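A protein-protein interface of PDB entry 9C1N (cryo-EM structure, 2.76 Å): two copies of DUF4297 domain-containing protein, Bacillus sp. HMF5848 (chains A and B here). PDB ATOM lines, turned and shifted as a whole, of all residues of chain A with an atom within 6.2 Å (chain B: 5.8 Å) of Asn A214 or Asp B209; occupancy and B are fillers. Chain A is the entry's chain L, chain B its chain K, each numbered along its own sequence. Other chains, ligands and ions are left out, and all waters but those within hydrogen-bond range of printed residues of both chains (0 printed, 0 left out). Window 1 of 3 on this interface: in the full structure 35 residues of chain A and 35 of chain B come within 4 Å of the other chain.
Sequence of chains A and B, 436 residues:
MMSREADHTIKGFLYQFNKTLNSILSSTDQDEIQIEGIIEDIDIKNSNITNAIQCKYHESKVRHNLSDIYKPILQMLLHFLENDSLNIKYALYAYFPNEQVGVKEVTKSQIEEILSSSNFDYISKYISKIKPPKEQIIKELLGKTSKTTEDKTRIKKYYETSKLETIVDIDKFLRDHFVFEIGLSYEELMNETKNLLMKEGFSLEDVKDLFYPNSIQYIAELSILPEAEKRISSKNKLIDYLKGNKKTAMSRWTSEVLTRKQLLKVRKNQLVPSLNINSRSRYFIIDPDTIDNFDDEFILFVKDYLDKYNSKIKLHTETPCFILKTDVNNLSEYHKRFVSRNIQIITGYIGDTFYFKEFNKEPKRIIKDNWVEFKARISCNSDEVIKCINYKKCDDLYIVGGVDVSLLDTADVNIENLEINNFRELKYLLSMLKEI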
ATOM      1  N   ASP A 209      24.828 -17.735  -0.663  1.00  0.00           N
ATOM      2  CA  ASP A 209      25.464 -17.138   0.508  1.00  0.00           C
ATOM      3  C   ASP A 209      26.074 -18.177   1.446  1.00  0.00           C
ATOM      4  O   ASP A 209      27.208 -18.005   1.905  1.00  0.00           O
ATOM      5  CB  ASP A 209      24.450 -16.275   1.267  1.00  0.00           C
ATOM      6  CG  ASP A 209      23.946 -15.108   0.441  1.00  0.00           C
ATOM      7  OD1 ASP A 209      24.613 -14.752  -0.556  1.00  0.00           O
ATOM      8  OD2 ASP A 209      22.889 -14.545   0.789  1.00  0.00           O
ATOM      9  N   LEU A 210      25.346 -19.251   1.746  1.00  0.00           N
ATOM     10  CA  LEU A 210      25.754 -20.204   2.770  1.00  0.00           C
ATOM     11  C   LEU A 210      26.086 -21.583   2.222  1.00  0.00           C
ATOM     12  O   LEU A 210      27.169 -22.109   2.494  1.00  0.00           O
ATOM     13  CB  LEU A 210      24.649 -20.326   3.831  1.00  0.00           C
ATOM     14  CG  LEU A 210      24.947 -21.216   5.040  1.00  0.00           C
ATOM     15  CD1 LEU A 210      25.650 -20.428   6.134  1.00  0.00           C
ATOM     16  CD2 LEU A 210      23.672 -21.855   5.567  1.00  0.00           C
ATOM     17  N   PHE A 211      25.175 -22.187   1.455  1.00  0.00           N
ATOM     18  CA  PHE A 211      25.297 -23.606   1.127  1.00  0.00           C
ATOM     19  C   PHE A 211      26.507 -23.885   0.242  1.00  0.00           C
ATOM     20  O   PHE A 211      27.301 -24.787   0.534  1.00  0.00           O
ATOM     21  CB  PHE A 211      24.012 -24.096   0.461  1.00  0.00           C
ATOM     22  CG  PHE A 211      22.866 -24.255   1.416  1.00  0.00           C
ATOM     23  CD1 PHE A 211      22.994 -25.051   2.542  1.00  0.00           C
ATOM     24  CD2 PHE A 211      21.666 -23.600   1.198  1.00  0.00           C
ATOM     25  CE1 PHE A 211      21.945 -25.199   3.427  1.00  0.00           C
ATOM     26  CE2 PHE A 211      20.614 -23.743   2.083  1.00  0.00           C
ATOM     27  CZ  PHE A 211      20.754 -24.545   3.197  1.00  0.00           C
ATOM     28  N   TYR A 212      26.660 -23.138  -0.851  1.00  0.00           N
ATOM     29  CA  TYR A 212      27.784 -23.384  -1.752  1.00  0.00           C
ATOM     30  C   TYR A 212      29.138 -23.120  -1.101  1.00  0.00           C
ATOM     31  O   TYR A 212      30.032 -23.977  -1.224  1.00  0.00           O
ATOM     32  CB  TYR A 212      27.606 -22.567  -3.038  1.00  0.00           C
ATOM     33  CG  TYR A 212      28.739 -22.724  -4.029  1.00  0.00           C
ATOM     34  CD1 TYR A 212      28.854 -23.870  -4.805  1.00  0.00           C
ATOM     35  CD2 TYR A 212      29.691 -21.726  -4.189  1.00  0.00           C
ATOM     36  CE1 TYR A 212      29.887 -24.018  -5.711  1.00  0.00           C
ATOM     37  CE2 TYR A 212      30.726 -21.864  -5.093  1.00  0.00           C
ATOM     38  CZ  TYR A 212      30.819 -23.012  -5.852  1.00  0.00           C
ATOM     39  OH  TYR A 212      31.849 -23.155  -6.754  1.00  0.00           O
ATOM     40  N   PRO A 213      29.379 -21.980  -0.432  1.00  0.00           N
ATOM     41  CA  PRO A 213      30.681 -21.809   0.235  1.00  0.00           C
ATOM     42  C   PRO A 213      30.947 -22.844   1.314  1.00  0.00           C
ATOM     43  O   PRO A 213      32.083 -23.317   1.444  1.00  0.00           O
ATOM     44  CB  PRO A 213      30.595 -20.389   0.814  1.00  0.00           C
ATOM     45  CG  PRO A 213      29.557 -19.708  -0.005  1.00  0.00           C
ATOM     46  CD  PRO A 213      28.550 -20.768  -0.303  1.00  0.00           C
ATOM     47  N   ASN A 214      29.923 -23.218   2.088  1.00  0.00           N
ATOM     48  CA  ASN A 214      30.112 -24.237   3.116  1.00  0.00           C
ATOM     49  C   ASN A 214      30.466 -25.582   2.498  1.00  0.00           C
ATOM     50  O   ASN A 214      31.341 -26.294   3.003  1.00  0.00           O
ATOM     51  CB  ASN A 214      28.858 -24.360   3.980  1.00  0.00           C
ATOM     52  CG  ASN A 214      28.896 -23.454   5.193  1.00  0.00           C
ATOM     53  OD1 ASN A 214      29.962 -23.174   5.738  1.00  0.00           O
ATOM     54  ND2 ASN A 214      27.727 -22.997   5.625  1.00  0.00           N
ATOM     55  N   SER A 215      29.796 -25.947   1.404  1.00  0.00           N
ATOM     56  CA  SER A 215      30.103 -27.206   0.734  1.00  0.00           C
ATOM     57  C   SER A 215      31.513 -27.194   0.155  1.00  0.00           C
ATOM     58  O   SER A 215      32.234 -28.194   0.246  1.00  0.00           O
ATOM     59  CB  SER A 215      29.070 -27.481  -0.357  1.00  0.00           C
ATOM     60  OG  SER A 215      27.763 -27.552   0.183  1.00  0.00           O
ATOM     61  N   ILE A 216      31.924 -26.072  -0.443  1.00  0.00           N
ATOM     62  CA  ILE A 216      33.275 -25.981  -0.991  1.00  0.00           C
ATOM     63  C   ILE A 216      34.311 -26.096   0.121  1.00  0.00           C
ATOM     64  O   ILE A 216      35.326 -26.790  -0.023  1.00  0.00           O
ATOM     65  CB  ILE A 216      33.444 -24.677  -1.793  1.00  0.00           C
ATOM     66  CG1 ILE A 216      32.557 -24.700  -3.039  1.00  0.00           C
ATOM     67  CG2 ILE A 216      34.900 -24.474  -2.186  1.00  0.00           C
ATOM     68  CD1 ILE A 216      32.896 -25.809  -4.011  1.00  0.00           C
ATOM     69  N   GLN A 217      34.070 -25.421   1.250  1.00  0.00           N
ATOM     70  CA  GLN A 217      34.985 -25.520   2.382  1.00  0.00           C
ATOM     71  C   GLN A 217      35.040 -26.941   2.925  1.00  0.00           C
ATOM     72  O   GLN A 217      36.111 -27.427   3.302  1.00  0.00           O
ATOM     73  CB  GLN A 217      34.568 -24.540   3.479  1.00  0.00           C
ATOM     74  CG  GLN A 217      35.490 -24.527   4.689  1.00  0.00           C
ATOM     75  CD  GLN A 217      36.878 -24.012   4.361  1.00  0.00           C
ATOM     76  OE1 GLN A 217      37.057 -23.224   3.433  1.00  0.00           O
ATOM     77  NE2 GLN A 217      37.869 -24.457   5.123  1.00  0.00           N
ATOM     78  N   TYR A 218      33.893 -27.621   2.980  1.00  0.00           N
ATOM     79  CA  TYR A 218      33.860 -29.003   3.446  1.00  0.00           C
ATOM     80  C   TYR A 218      34.660 -29.915   2.524  1.00  0.00           C
ATOM     81  O   TYR A 218      35.425 -30.770   2.991  1.00  0.00           O
ATOM     82  CB  TYR A 218      32.405 -29.466   3.552  1.00  0.00           C
ATOM     83  CG  TYR A 218      32.213 -30.907   3.964  1.00  0.00           C
ATOM     84  CD1 TYR A 218      32.361 -31.296   5.288  1.00  0.00           C
ATOM     85  CD2 TYR A 218      31.857 -31.873   3.033  1.00  0.00           C
ATOM     86  CE1 TYR A 218      32.176 -32.611   5.673  1.00  0.00           C
ATOM     87  CE2 TYR A 218      31.669 -33.191   3.406  1.00  0.00           C
ATOM     88  CZ  TYR A 218      31.828 -33.553   4.727  1.00  0.00           C
ATOM     89  OH  TYR A 218      31.644 -34.863   5.104  1.00  0.00           O
ATOM     90  N   ILE A 219      34.507 -29.738   1.209  1.00  0.00           N
ATOM     91  CA  ILE A 219      35.270 -30.537   0.252  1.00  0.00           C
ATOM     92  C   ILE A 219      36.762 -30.272   0.408  1.00  0.00           C
ATOM     93  O   ILE A 219      37.576 -31.204   0.409  1.00  0.00           O
ATOM     94  CB  ILE A 219      34.795 -30.257  -1.186  1.00  0.00           C
ATOM     95  CG1 ILE A 219      33.315 -30.610  -1.351  1.00  0.00           C
ATOM     96  CG2 ILE A 219      35.640 -31.028  -2.190  1.00  0.00           C
ATOM     97  CD1 ILE A 219      32.973 -32.029  -0.968  1.00  0.00           C
ATOM     98  N   LEU A 238      26.424 -34.654   3.770  1.00  0.00           N
ATOM     99  CA  LEU A 238      26.558 -33.254   3.384  1.00  0.00           C
ATOM    100  C   LEU A 238      25.249 -32.499   3.579  1.00  0.00           C
ATOM    101  O   LEU A 238      25.245 -31.359   4.061  1.00  0.00           O
ATOM    102  CB  LEU A 238      27.024 -33.152   1.931  1.00  0.00           C
ATOM    103  CG  LEU A 238      27.035 -31.754   1.313  1.00  0.00           C
ATOM    104  CD1 LEU A 238      28.153 -30.910   1.907  1.00  0.00           C
ATOM    105  CD2 LEU A 238      27.164 -31.837  -0.200  1.00  0.00           C
ATOM    106  N   TYR A 241      24.762 -31.918   7.283  1.00  0.00           N
ATOM    107  CA  TYR A 241      25.674 -30.886   7.770  1.00  0.00           C
ATOM    108  C   TYR A 241      25.190 -29.496   7.374  1.00  0.00           C
ATOM    109  O   TYR A 241      25.176 -28.569   8.196  1.00  0.00           O
ATOM    110  CB  TYR A 241      27.082 -31.154   7.234  1.00  0.00           C
ATOM    111  CG  TYR A 241      28.069 -30.025   7.432  1.00  0.00           C
ATOM    112  CD1 TYR A 241      28.654 -29.800   8.671  1.00  0.00           C
ATOM    113  CD2 TYR A 241      28.431 -29.200   6.376  1.00  0.00           C
ATOM    114  CE1 TYR A 241      29.564 -28.774   8.855  1.00  0.00           C
ATOM    115  CE2 TYR A 241      29.338 -28.172   6.550  1.00  0.00           C
ATOM    116  CZ  TYR A 241      29.903 -27.965   7.790  1.00  0.00           C
ATOM    117  OH  TYR A 241      30.806 -26.942   7.968  1.00  0.00           O
ATOM    118  N   LEU A 242      24.775 -29.336   6.113  1.00  0.00           N
ATOM    119  CA  LEU A 242      24.272 -28.044   5.657  1.00  0.00           C
ATOM    120  C   LEU A 242      23.000 -27.650   6.398  1.00  0.00           C
ATOM    121  O   LEU A 242      22.838 -26.488   6.792  1.00  0.00           O
ATOM    122  CB  LEU A 242      24.027 -28.078   4.149  1.00  0.00           C
ATOM    123  CG  LEU A 242      25.268 -28.168   3.257  1.00  0.00           C
ATOM    124  CD1 LEU A 242      24.870 -28.284   1.793  1.00  0.00           C
ATOM    125  CD2 LEU A 242      26.176 -26.970   3.477  1.00  0.00           C
ATOM    126  N   ASN A 245      23.919 -26.580   9.956  1.00  0.00           N
ATOM    127  CA  ASN A 245      24.504 -25.244   9.947  1.00  0.00           C
ATOM    128  C   ASN A 245      23.437 -24.178   9.738  1.00  0.00           C
ATOM    129  O   ASN A 245      23.433 -23.149  10.427  1.00  0.00           O
ATOM    130  CB  ASN A 245      25.578 -25.141   8.866  1.00  0.00           C
ATOM    131  CG  ASN A 245      26.874 -25.813   9.265  1.00  0.00           C
ATOM    132  OD1 ASN A 245      26.994 -26.359  10.361  1.00  0.00           O
ATOM    133  ND2 ASN A 245      27.859 -25.767   8.376  1.00  0.00           N
ATOM    134  N   THR A 248      21.308 -23.871  12.979  1.00  0.00           N
ATOM    135  CA  THR A 248      22.040 -23.190  14.042  1.00  0.00           C
ATOM    136  C   THR A 248      22.163 -21.700  13.755  1.00  0.00           C
ATOM    137  O   THR A 248      21.967 -20.868  14.651  1.00  0.00           O
ATOM    138  CB  THR A 248      23.424 -23.817  14.216  1.00  0.00           C
ATOM    139  OG1 THR A 248      23.292 -25.237  14.361  1.00  0.00           O
ATOM    140  CG2 THR A 248      24.115 -23.249  15.446  1.00  0.00           C
ATOM    141  N   ALA A 249      22.478 -21.342  12.507  1.00  0.00           N
ATOM    142  CA  ALA A 249      22.567 -19.933  12.144  1.00  0.00           C
ATOM    143  C   ALA A 249      21.221 -19.239  12.303  1.00  0.00           C
ATOM    144  O   ALA A 249      21.152 -18.120  12.819  1.00  0.00           O
ATOM    145  CB  ALA A 249      23.083 -19.789  10.713  1.00  0.00           C
ATOM    146  N   ARG A 252      20.525 -18.800  16.144  1.00  0.00           N
ATOM    147  CA  ARG A 252      21.397 -17.798  16.748  1.00  0.00           C
ATOM    148  C   ARG A 252      21.052 -16.397  16.262  1.00  0.00           C
ATOM    149  O   ARG A 252      21.073 -15.437  17.041  1.00  0.00           O
ATOM    150  CB  ARG A 252      22.857 -18.128  16.441  1.00  0.00           C
ATOM    151  CG  ARG A 252      23.868 -17.210  17.107  1.00  0.00           C
ATOM    152  CD  ARG A 252      25.291 -17.626  16.765  1.00  0.00           C
ATOM    153  NE  ARG A 252      25.569 -17.511  15.338  1.00  0.00           N
ATOM    154  CZ  ARG A 252      25.641 -18.536  14.500  1.00  0.00           C
ATOM    155  NH1 ARG A 252      25.452 -19.779  14.913  1.00  0.00           N
ATOM    156  NH2 ARG A 252      25.905 -18.309  13.217  1.00  0.00           N
ATOM    157  N   TRP A 253      20.731 -16.258  14.974  1.00  0.00           N
ATOM    158  CA  TRP A 253      20.457 -14.950  14.399  1.00  0.00           C
ATOM    159  C   TRP A 253      19.065 -14.444  14.755  1.00  0.00           C
ATOM    160  O   TRP A 253      18.867 -13.229  14.875  1.00  0.00           O
ATOM    161  CB  TRP A 253      20.659 -15.025  12.886  1.00  0.00           C
ATOM    162  CG  TRP A 253      22.110 -15.182  12.528  1.00  0.00           C
ATOM    163  CD1 TRP A 253      23.175 -15.005  13.361  1.00  0.00           C
ATOM    164  CD2 TRP A 253      22.655 -15.567  11.259  1.00  0.00           C
ATOM    165  NE1 TRP A 253      24.348 -15.240  12.689  1.00  0.00           N
ATOM    166  CE2 TRP A 253      24.057 -15.586  11.396  1.00  0.00           C
ATOM    167  CE3 TRP A 253      22.095 -15.883  10.017  1.00  0.00           C
ATOM    168  CZ2 TRP A 253      24.906 -15.914  10.342  1.00  0.00           C
ATOM    169  CZ3 TRP A 253      22.943 -16.205   8.972  1.00  0.00           C
ATOM    170  CH2 TRP A 253      24.331 -16.222   9.142  1.00  0.00           C
ATOM    171  N   LEU B 204      32.029 -16.249  17.341  1.00  0.00           N
ATOM    172  CA  LEU B 204      32.765 -17.448  16.951  1.00  0.00           C
ATOM    173  C   LEU B 204      31.917 -18.359  16.071  1.00  0.00           C
ATOM    174  O   LEU B 204      32.398 -18.876  15.055  1.00  0.00           O
ATOM    175  CB  LEU B 204      33.243 -18.197  18.195  1.00  0.00           C
ATOM    176  CG  LEU B 204      33.869 -19.574  17.968  1.00  0.00           C
ATOM    177  CD1 LEU B 204      35.123 -19.462  17.114  1.00  0.00           C
ATOM    178  CD2 LEU B 204      34.178 -20.250  19.295  1.00  0.00           C
ATOM    179  N   GLU B 205      30.653 -18.569  16.446  1.00  0.00           N
ATOM    180  CA  GLU B 205      29.774 -19.411  15.641  1.00  0.00           C
ATOM    181  C   GLU B 205      29.522 -18.795  14.271  1.00  0.00           C
ATOM    182  O   GLU B 205      29.502 -19.505  13.256  1.00  0.00           O
ATOM    183  CB  GLU B 205      28.453 -19.644  16.376  1.00  0.00           C
ATOM    184  CG  GLU B 205      28.568 -20.553  17.588  1.00  0.00           C
ATOM    185  CD  GLU B 205      28.821 -21.998  17.211  1.00  0.00           C
ATOM    186  OE1 GLU B 205      28.356 -22.423  16.132  1.00  0.00           O
ATOM    187  OE2 GLU B 205      29.485 -22.711  17.992  1.00  0.00           O
ATOM    188  N   ASP B 206      29.323 -17.475  14.222  1.00  0.00           N
ATOM    189  CA  ASP B 206      29.102 -16.806  12.945  1.00  0.00           C
ATOM    190  C   ASP B 206      30.315 -16.944  12.035  1.00  0.00           C
ATOM    191  O   ASP B 206      30.175 -17.217  10.836  1.00  0.00           O
ATOM    192  CB  ASP B 206      28.772 -15.332  13.176  1.00  0.00           C
ATOM    193  CG  ASP B 206      27.379 -15.128  13.730  1.00  0.00           C
ATOM    194  OD1 ASP B 206      26.455 -15.838  13.284  1.00  0.00           O
ATOM    195  OD2 ASP B 206      27.207 -14.258  14.610  1.00  0.00           O
ATOM    196  N   VAL B 207      31.516 -16.764  12.587  1.00  0.00           N
ATOM    197  CA  VAL B 207      32.732 -16.928  11.796  1.00  0.00           C
ATOM    198  C   VAL B 207      32.860 -18.366  11.309  1.00  0.00           C
ATOM    199  O   VAL B 207      33.169 -18.616  10.138  1.00  0.00           O
ATOM    200  CB  VAL B 207      33.964 -16.494  12.613  1.00  0.00           C
ATOM    201  CG1 VAL B 207      35.245 -16.965  11.944  1.00  0.00           C
ATOM    202  CG2 VAL B 207      33.976 -14.985  12.792  1.00  0.00           C
ATOM    203  N   LYS B 208      32.610 -19.331  12.198  1.00  0.00           N
ATOM    204  CA  LYS B 208      32.772 -20.736  11.835  1.00  0.00           C
ATOM    205  C   LYS B 208      31.801 -21.147  10.735  1.00  0.00           C
ATOM    206  O   LYS B 208      32.171 -21.892   9.819  1.00  0.00           O
ATOM    207  CB  LYS B 208      32.585 -21.617  13.070  1.00  0.00           C
ATOM    208  CG  LYS B 208      33.843 -21.797  13.903  1.00  0.00           C
ATOM    209  CD  LYS B 208      33.568 -22.634  15.141  1.00  0.00           C
ATOM    210  CE  LYS B 208      34.857 -23.008  15.854  1.00  0.00           C
ATOM    211  NZ  LYS B 208      34.597 -23.716  17.137  1.00  0.00           N
ATOM    212  N   ASP B 209      30.557 -20.675  10.803  1.00  0.00           N
ATOM    213  CA  ASP B 209      29.531 -21.137   9.876  1.00  0.00           C
ATOM    214  C   ASP B 209      29.502 -20.341   8.575  1.00  0.00           C
ATOM    215  O   ASP B 209      29.447 -20.929   7.489  1.00  0.00           O
ATOM    216  CB  ASP B 209      28.157 -21.087  10.552  1.00  0.00           C
ATOM    217  CG  ASP B 209      28.066 -22.009  11.753  1.00  0.00           C
ATOM    218  OD1 ASP B 209      28.900 -22.932  11.861  1.00  0.00           O
ATOM    219  OD2 ASP B 209      27.158 -21.811  12.590  1.00  0.00           O
ATOM    220  N   LEU B 210      29.539 -19.012   8.657  1.00  0.00           N
ATOM    221  CA  LEU B 210      29.320 -18.155   7.499  1.00  0.00           C
ATOM    222  C   LEU B 210      30.553 -17.367   7.082  1.00  0.00           C
ATOM    223  O   LEU B 210      30.947 -17.414   5.913  1.00  0.00           O
ATOM    224  CB  LEU B 210      28.164 -17.184   7.786  1.00  0.00           C
ATOM    225  CG  LEU B 210      27.729 -16.265   6.644  1.00  0.00           C
ATOM    226  CD1 LEU B 210      26.757 -16.972   5.714  1.00  0.00           C
ATOM    227  CD2 LEU B 210      27.120 -14.980   7.188  1.00  0.00           C
ATOM    228  N   PHE B 211      31.172 -16.637   8.012  1.00  0.00           N
ATOM    229  CA  PHE B 211      32.177 -15.645   7.633  1.00  0.00           C
ATOM    230  C   PHE B 211      33.437 -16.297   7.075  1.00  0.00           C
ATOM    231  O   PHE B 211      33.939 -15.891   6.021  1.00  0.00           O
ATOM    232  CB  PHE B 211      32.506 -14.757   8.831  1.00  0.00           C
ATOM    233  CG  PHE B 211      31.406 -13.799   9.188  1.00  0.00           C
ATOM    234  CD1 PHE B 211      30.954 -12.872   8.265  1.00  0.00           C
ATOM    235  CD2 PHE B 211      30.817 -13.833  10.440  1.00  0.00           C
ATOM    236  CE1 PHE B 211      29.939 -11.991   8.585  1.00  0.00           C
ATOM    237  CE2 PHE B 211      29.801 -12.954  10.766  1.00  0.00           C
ATOM    238  CZ  PHE B 211      29.363 -12.034   9.837  1.00  0.00           C
ATOM    239  N   TYR B 212      33.975 -17.298   7.772  1.00  0.00           N
ATOM    240  CA  TYR B 212      35.198 -17.943   7.297  1.00  0.00           C
ATOM    241  C   TYR B 212      35.015 -18.662   5.965  1.00  0.00           C
ATOM    242  O   TYR B 212      35.857 -18.475   5.070  1.00  0.00           O
ATOM    243  CB  TYR B 212      35.742 -18.890   8.373  1.00  0.00           C
ATOM    244  CG  TYR B 212      37.025 -19.582   7.977  1.00  0.00           C
ATOM    245  CD1 TYR B 212      38.236 -18.903   7.994  1.00  0.00           C
ATOM    246  CD2 TYR B 212      37.024 -20.910   7.572  1.00  0.00           C
ATOM    247  CE1 TYR B 212      39.412 -19.530   7.630  1.00  0.00           C
ATOM    248  CE2 TYR B 212      38.194 -21.544   7.201  1.00  0.00           C
ATOM    249  CZ  TYR B 212      39.385 -20.850   7.235  1.00  0.00           C
ATOM    250  OH  TYR B 212      40.553 -21.480   6.869  1.00  0.00           O
ATOM    251  N   PRO B 213      33.990 -19.506   5.766  1.00  0.00           N
ATOM    252  CA  PRO B 213      33.824 -20.120   4.435  1.00  0.00           C
ATOM    253  C   PRO B 213      33.592 -19.104   3.331  1.00  0.00           C
ATOM    254  O   PRO B 213      34.115 -19.273   2.222  1.00  0.00           O
ATOM    255  CB  PRO B 213      32.612 -21.045   4.624  1.00  0.00           C
ATOM    256  CG  PRO B 213      32.553 -21.299   6.088  1.00  0.00           C
ATOM    257  CD  PRO B 213      32.988 -20.018   6.718  1.00  0.00           C
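Of the 19 printed residues of chain A, 7 touch a printed residue of chain B.
Hydrophobic or aromatic side chains of chain A that line the printed part of chain B: Leu A210, Pro A213 and Trp A253.
Printed residues of chain B that touch a printed residue of chain A: Glu B205, Asp B206, Asp B209, Leu B210, Tyr B212 and Pro B213.
Hydrophobic or aromatic side chains of chain B within 4 Å of the printed part of chain A: Leu B210, Tyr B212 and Pro B213.
Among the printed residues, 11 pairs touch across the chains.
OD1 of Asp B206 is in salt-bridge range of NH2 of Arg A252 (2.5 Å).
The backbone carbonyl oxygen (O) of Asp B209 lies close to the side-chain amide oxygen (OD1) of Asn A214 (2.9 Å).
OD2 of Asp B209 is in salt-bridge range of NH1 of Arg A252, 3.5 Å away.
NE1 of Trp A253 sits close to OD1 of Asp B206.
The backbone NH (N) of Phe B211 is in hydrogen-bond range of the backbone carbonyl oxygen (O) of Asp B206, 3.1 Å away.
The backbone carbonyl oxygen (O) of Val B207 sits at hydrogen-bond distance from the backbone NH (N) of Tyr B212, at 2.8 Å.
The side-chain amide nitrogen (ND2) of Asn A214 sits close to the backbone carbonyl oxygen (O) of Leu A210 (3.3 Å).
O of Asp A209 touches CD1 of Leu B210 (3.97 Å).
CD1 of Leu B210 touches CD1 of Leu A210, 3.7 Å away.
Pro A213 touches Pro B213 (O to CB, 3.9 Å).
OD1 of Asn A214 touches CG of Pro B213, at 3.2 Å.
Tyr B212 touches Gln A217 (CE2 to NE2, 3.6 Å).
NH1 of Arg A252 touches CB of Glu B205, 3.3 Å away.
CH2 of Trp A253 touches CD2 of Leu B210 (3.6 Å).
Of chain B, only Asp B209 (2.9 Å) and Pro B213 (3.2 Å) come within 4 Å of Asn A214.
Ala A249 touches none of the printed residues of chain B.
Printed residues of chain B within 4 Å of Arg A252: Glu B205, Asp B206 and Asp B209.
Of the printed residues of chain B, Trp A253 touches Asp B206 (2.3 Å) and Leu B210 (3.6 Å).
Of the printed residues of chain A, Glu B205 touches Arg A252 (3.3 Å).
Asp B209 touches two residues of chain A.
Printed residues of chain A within 4 Å of Tyr B212: Gln A217.
Asp A209 touches Leu B210, but with the chains exchanged Leu A210 does not touch Asp B209 (4.1 Å).
Leu A210 touches its own counterpart, Leu B210.
Pro B213 touches its own counterpart, Pro A213.
Of the 11 pairs that touch across the chains among the printed residues, 2 have their exchanged pair printed and touching as well.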
